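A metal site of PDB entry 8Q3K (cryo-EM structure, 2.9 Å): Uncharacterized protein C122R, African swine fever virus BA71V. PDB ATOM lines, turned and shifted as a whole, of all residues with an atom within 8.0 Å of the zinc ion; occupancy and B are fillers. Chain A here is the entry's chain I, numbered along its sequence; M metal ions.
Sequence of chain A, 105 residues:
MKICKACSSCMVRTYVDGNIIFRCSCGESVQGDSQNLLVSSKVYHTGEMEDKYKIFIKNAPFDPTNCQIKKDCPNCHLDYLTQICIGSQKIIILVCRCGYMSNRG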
ATOM      1  N   LYS A   2     -19.730 -16.942  -9.432  1.00  0.00           N
ATOM      2  CA  LYS A   2     -21.068 -17.164  -8.922  1.00  0.00           C
ATOM      3  C   LYS A   2     -21.047 -17.100  -7.403  1.00  0.00           C
ATOM      4  O   LYS A   2     -20.154 -17.673  -6.770  1.00  0.00           O
ATOM      5  CB  LYS A   2     -21.629 -18.513  -9.381  1.00  0.00           C
ATOM      6  CG  LYS A   2     -22.499 -18.457 -10.627  1.00  0.00           C
ATOM      7  CD  LYS A   2     -23.636 -19.449 -10.548  1.00  0.00           C
ATOM      8  CE  LYS A   2     -24.298 -19.665 -11.897  1.00  0.00           C
ATOM      9  NZ  LYS A   2     -24.863 -18.396 -12.451  1.00  0.00           N
ATOM     10  N   ILE A   3     -22.024 -16.411  -6.827  1.00  0.00           N
ATOM     11  CA  ILE A   3     -22.176 -16.300  -5.374  1.00  0.00           C
ATOM     12  C   ILE A   3     -23.590 -16.721  -5.032  1.00  0.00           C
ATOM     13  O   ILE A   3     -24.563 -16.098  -5.473  1.00  0.00           O
ATOM     14  CB  ILE A   3     -21.881 -14.877  -4.883  1.00  0.00           C
ATOM     15  CG1 ILE A   3     -22.452 -13.844  -5.851  1.00  0.00           C
ATOM     16  CG2 ILE A   3     -20.385 -14.678  -4.693  1.00  0.00           C
ATOM     17  CD1 ILE A   3     -22.323 -12.419  -5.372  1.00  0.00           C
ATOM     18  N   CYS A   4     -23.709 -17.772  -4.218  1.00  0.00           N
ATOM     19  CA  CYS A   4     -25.032 -18.254  -3.827  1.00  0.00           C
ATOM     20  C   CYS A   4     -25.754 -17.189  -3.021  1.00  0.00           C
ATOM     21  O   CYS A   4     -25.187 -16.564  -2.115  1.00  0.00           O
ATOM     22  CB  CYS A   4     -24.907 -19.546  -3.017  1.00  0.00           C
ATOM     23  SG  CYS A   4     -23.490 -19.616  -1.914  1.00  0.00           S
ATOM     24  N   LYS A   5     -27.031 -16.979  -3.351  1.00  0.00           N
ATOM     25  CA  LYS A   5     -27.815 -15.943  -2.691  1.00  0.00           C
ATOM     26  C   LYS A   5     -27.943 -16.199  -1.193  1.00  0.00           C
ATOM     27  O   LYS A   5     -28.112 -15.253  -0.409  1.00  0.00           O
ATOM     28  CB  LYS A   5     -29.204 -15.850  -3.333  1.00  0.00           C
ATOM     29  CG  LYS A   5     -29.216 -15.612  -4.860  1.00  0.00           C
ATOM     30  CD  LYS A   5     -28.144 -14.649  -5.405  1.00  0.00           C
ATOM     31  CE  LYS A   5     -28.058 -13.330  -4.652  1.00  0.00           C
ATOM     32  NZ  LYS A   5     -29.401 -12.717  -4.428  1.00  0.00           N
ATOM     33  N   ALA A   6     -27.867 -17.464  -0.769  1.00  0.00           N
ATOM     34  CA  ALA A   6     -27.920 -17.769   0.659  1.00  0.00           C
ATOM     35  C   ALA A   6     -26.734 -17.145   1.389  1.00  0.00           C
ATOM     36  O   ALA A   6     -26.903 -16.552   2.469  1.00  0.00           O
ATOM     37  CB  ALA A   6     -27.932 -19.280   0.885  1.00  0.00           C
ATOM     38  N   CYS A   7     -25.539 -17.261   0.828  1.00  0.00           N
ATOM     39  CA  CYS A   7     -24.346 -16.679   1.421  1.00  0.00           C
ATOM     40  C   CYS A   7     -23.387 -16.289   0.302  1.00  0.00           C
ATOM     41  O   CYS A   7     -23.160 -17.066  -0.620  1.00  0.00           O
ATOM     42  CB  CYS A   7     -23.669 -17.653   2.393  1.00  0.00           C
ATOM     43  SG  CYS A   7     -22.475 -18.792   1.642  1.00  0.00           S
ATOM     44  N   SER A   8     -22.834 -15.083   0.400  1.00  0.00           N
ATOM     45  CA  SER A   8     -21.875 -14.615  -0.588  1.00  0.00           C
ATOM     46  C   SER A   8     -20.594 -15.424  -0.471  1.00  0.00           C
ATOM     47  O   SER A   8     -19.800 -15.204   0.453  1.00  0.00           O
ATOM     48  CB  SER A   8     -21.606 -13.126  -0.404  1.00  0.00           C
ATOM     49  OG  SER A   8     -22.752 -12.358  -0.758  1.00  0.00           O
ATOM     50  N   SER A   9     -20.383 -16.352  -1.391  1.00  0.00           N
ATOM     51  CA  SER A   9     -19.203 -17.201  -1.377  1.00  0.00           C
ATOM     52  C   SER A   9     -19.020 -17.798  -2.762  1.00  0.00           C
ATOM     53  O   SER A   9     -19.988 -18.001  -3.506  1.00  0.00           O
ATOM     54  CB  SER A   9     -19.325 -18.314  -0.331  1.00  0.00           C
ATOM     55  OG  SER A   9     -18.171 -19.141  -0.328  1.00  0.00           O
ATOM     56  N   CYS A  10     -17.771 -18.082  -3.107  1.00  0.00           N
ATOM     57  CA  CYS A  10     -17.457 -18.636  -4.420  1.00  0.00           C
ATOM     58  C   CYS A  10     -18.125 -19.988  -4.597  1.00  0.00           C
ATOM     59  O   CYS A  10     -18.073 -20.846  -3.704  1.00  0.00           O
ATOM     60  CB  CYS A  10     -15.945 -18.767  -4.588  1.00  0.00           C
ATOM     61  SG  CYS A  10     -15.013 -17.250  -4.241  1.00  0.00           S
ATOM     62  N   MET A  11     -18.768 -20.178  -5.740  1.00  0.00           N
ATOM     63  CA  MET A  11     -19.408 -21.450  -6.091  1.00  0.00           C
ATOM     64  C   MET A  11     -18.372 -22.311  -6.807  1.00  0.00           C
ATOM     65  O   MET A  11     -17.953 -21.982  -7.920  1.00  0.00           O
ATOM     66  CB  MET A  11     -20.632 -21.209  -6.969  1.00  0.00           C
ATOM     67  CG  MET A  11     -21.749 -20.413  -6.310  1.00  0.00           C
ATOM     68  SD  MET A  11     -22.482 -21.219  -4.875  1.00  0.00           S
ATOM     69  CE  MET A  11     -23.328 -22.599  -5.653  1.00  0.00           C
ATOM     70  N   ARG A  23     -21.871 -25.445  -6.742  1.00  0.00           N
ATOM     71  CA  ARG A  23     -22.087 -25.769  -5.334  1.00  0.00           C
ATOM     72  C   ARG A  23     -21.256 -24.856  -4.450  1.00  0.00           C
ATOM     73  O   ARG A  23     -20.225 -24.319  -4.864  1.00  0.00           O
ATOM     74  CB  ARG A  23     -21.740 -27.242  -5.027  1.00  0.00           C
ATOM     75  CG  ARG A  23     -22.244 -28.235  -6.074  1.00  0.00           C
ATOM     76  CD  ARG A  23     -21.832 -29.659  -5.732  1.00  0.00           C
ATOM     77  NE  ARG A  23     -22.373 -30.100  -4.454  1.00  0.00           N
ATOM     78  CZ  ARG A  23     -22.158 -31.286  -3.920  1.00  0.00           C
ATOM     79  NH1 ARG A  23     -21.406 -32.198  -4.523  1.00  0.00           N
ATOM     80  NH2 ARG A  23     -22.714 -31.584  -2.741  1.00  0.00           N
ATOM     81  N   CYS A  24     -21.728 -24.689  -3.211  1.00  0.00           N
ATOM     82  CA  CYS A  24     -20.995 -23.976  -2.168  1.00  0.00           C
ATOM     83  C   CYS A  24     -20.879 -24.863  -0.934  1.00  0.00           C
ATOM     84  O   CYS A  24     -21.410 -25.971  -0.872  1.00  0.00           O
ATOM     85  CB  CYS A  24     -21.692 -22.659  -1.790  1.00  0.00           C
ATOM     86  SG  CYS A  24     -21.047 -21.888  -0.286  1.00  0.00           S
ATOM     87  N   SER A  25     -20.150 -24.346   0.058  1.00  0.00           N
ATOM     88  CA  SER A  25     -20.046 -25.054   1.337  1.00  0.00           C
ATOM     89  C   SER A  25     -21.395 -25.119   2.046  1.00  0.00           C
ATOM     90  O   SER A  25     -21.624 -26.032   2.845  1.00  0.00           O
ATOM     91  CB  SER A  25     -19.011 -24.379   2.226  1.00  0.00           C
ATOM     92  OG  SER A  25     -18.875 -25.057   3.463  1.00  0.00           O
ATOM     93  N   CYS A  26     -22.278 -24.170   1.772  1.00  0.00           N
ATOM     94  CA  CYS A  26     -23.588 -24.123   2.399  1.00  0.00           C
ATOM     95  C   CYS A  26     -24.656 -24.887   1.621  1.00  0.00           C
ATOM     96  O   CYS A  26     -25.775 -25.042   2.136  1.00  0.00           O
ATOM     97  CB  CYS A  26     -24.044 -22.668   2.558  1.00  0.00           C
ATOM     98  SG  CYS A  26     -24.579 -21.874   1.016  1.00  0.00           S
ATOM     99  N   GLY A  27     -24.350 -25.365   0.418  1.00  0.00           N
ATOM    100  CA  GLY A  27     -25.341 -26.047  -0.396  1.00  0.00           C
ATOM    101  C   GLY A  27     -26.042 -25.119  -1.355  1.00  0.00           C
ATOM    102  O   GLY A  27     -25.410 -24.254  -1.966  1.00  0.00           O
ATOM    103  N   GLU A  28     -27.359 -25.283  -1.503  1.00  0.00           N
ATOM    104  CA  GLU A  28     -28.179 -24.428  -2.360  1.00  0.00           C
ATOM    105  C   GLU A  28     -27.753 -24.511  -3.820  1.00  0.00           C
ATOM    106  O   GLU A  28     -28.176 -23.707  -4.658  1.00  0.00           O
ATOM    107  CB  GLU A  28     -28.154 -22.977  -1.831  1.00  0.00           C
ATOM    108  CG  GLU A  28     -28.588 -21.851  -2.767  1.00  0.00           C
ATOM    109  CD  GLU A  28     -27.469 -21.369  -3.685  1.00  0.00           C
ATOM    110  OE1 GLU A  28     -26.389 -21.987  -3.675  1.00  0.00           O
ATOM    111  OE2 GLU A  28     -27.683 -20.367  -4.399  1.00  0.00           O
ATOM    112  N   SER A  29     -26.979 -25.554  -4.160  1.00  0.00           N
ATOM    113  CA  SER A  29     -26.341 -25.661  -5.470  1.00  0.00           C
ATOM    114  C   SER A  29     -27.289 -25.276  -6.590  1.00  0.00           C
ATOM    115  O   SER A  29     -28.478 -25.603  -6.568  1.00  0.00           O
ATOM    116  CB  SER A  29     -25.849 -27.097  -5.672  1.00  0.00           C
ATOM    117  OG  SER A  29     -25.723 -27.401  -7.055  1.00  0.00           O
HETATM  118 ZN    ZN M   1     -22.891 -20.528   0.150  1.00  0.00          ZN
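The side-chain sulfur (SD) of Met 11 lies close to the backbone NH (N) of Cys 4 (3.7 Å).
Four residues have an atom within 4 Å of the zinc ion: Cys 4, Cys 7, Cys 24 and Cys 26.
Along chain A the residues within 4 Å of the zinc ion span positions 4 to 26.
The zinc ion is bound by SG of Cys 26, SG of Cys 7, SG of Cys 24 and SG of Cys 4.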
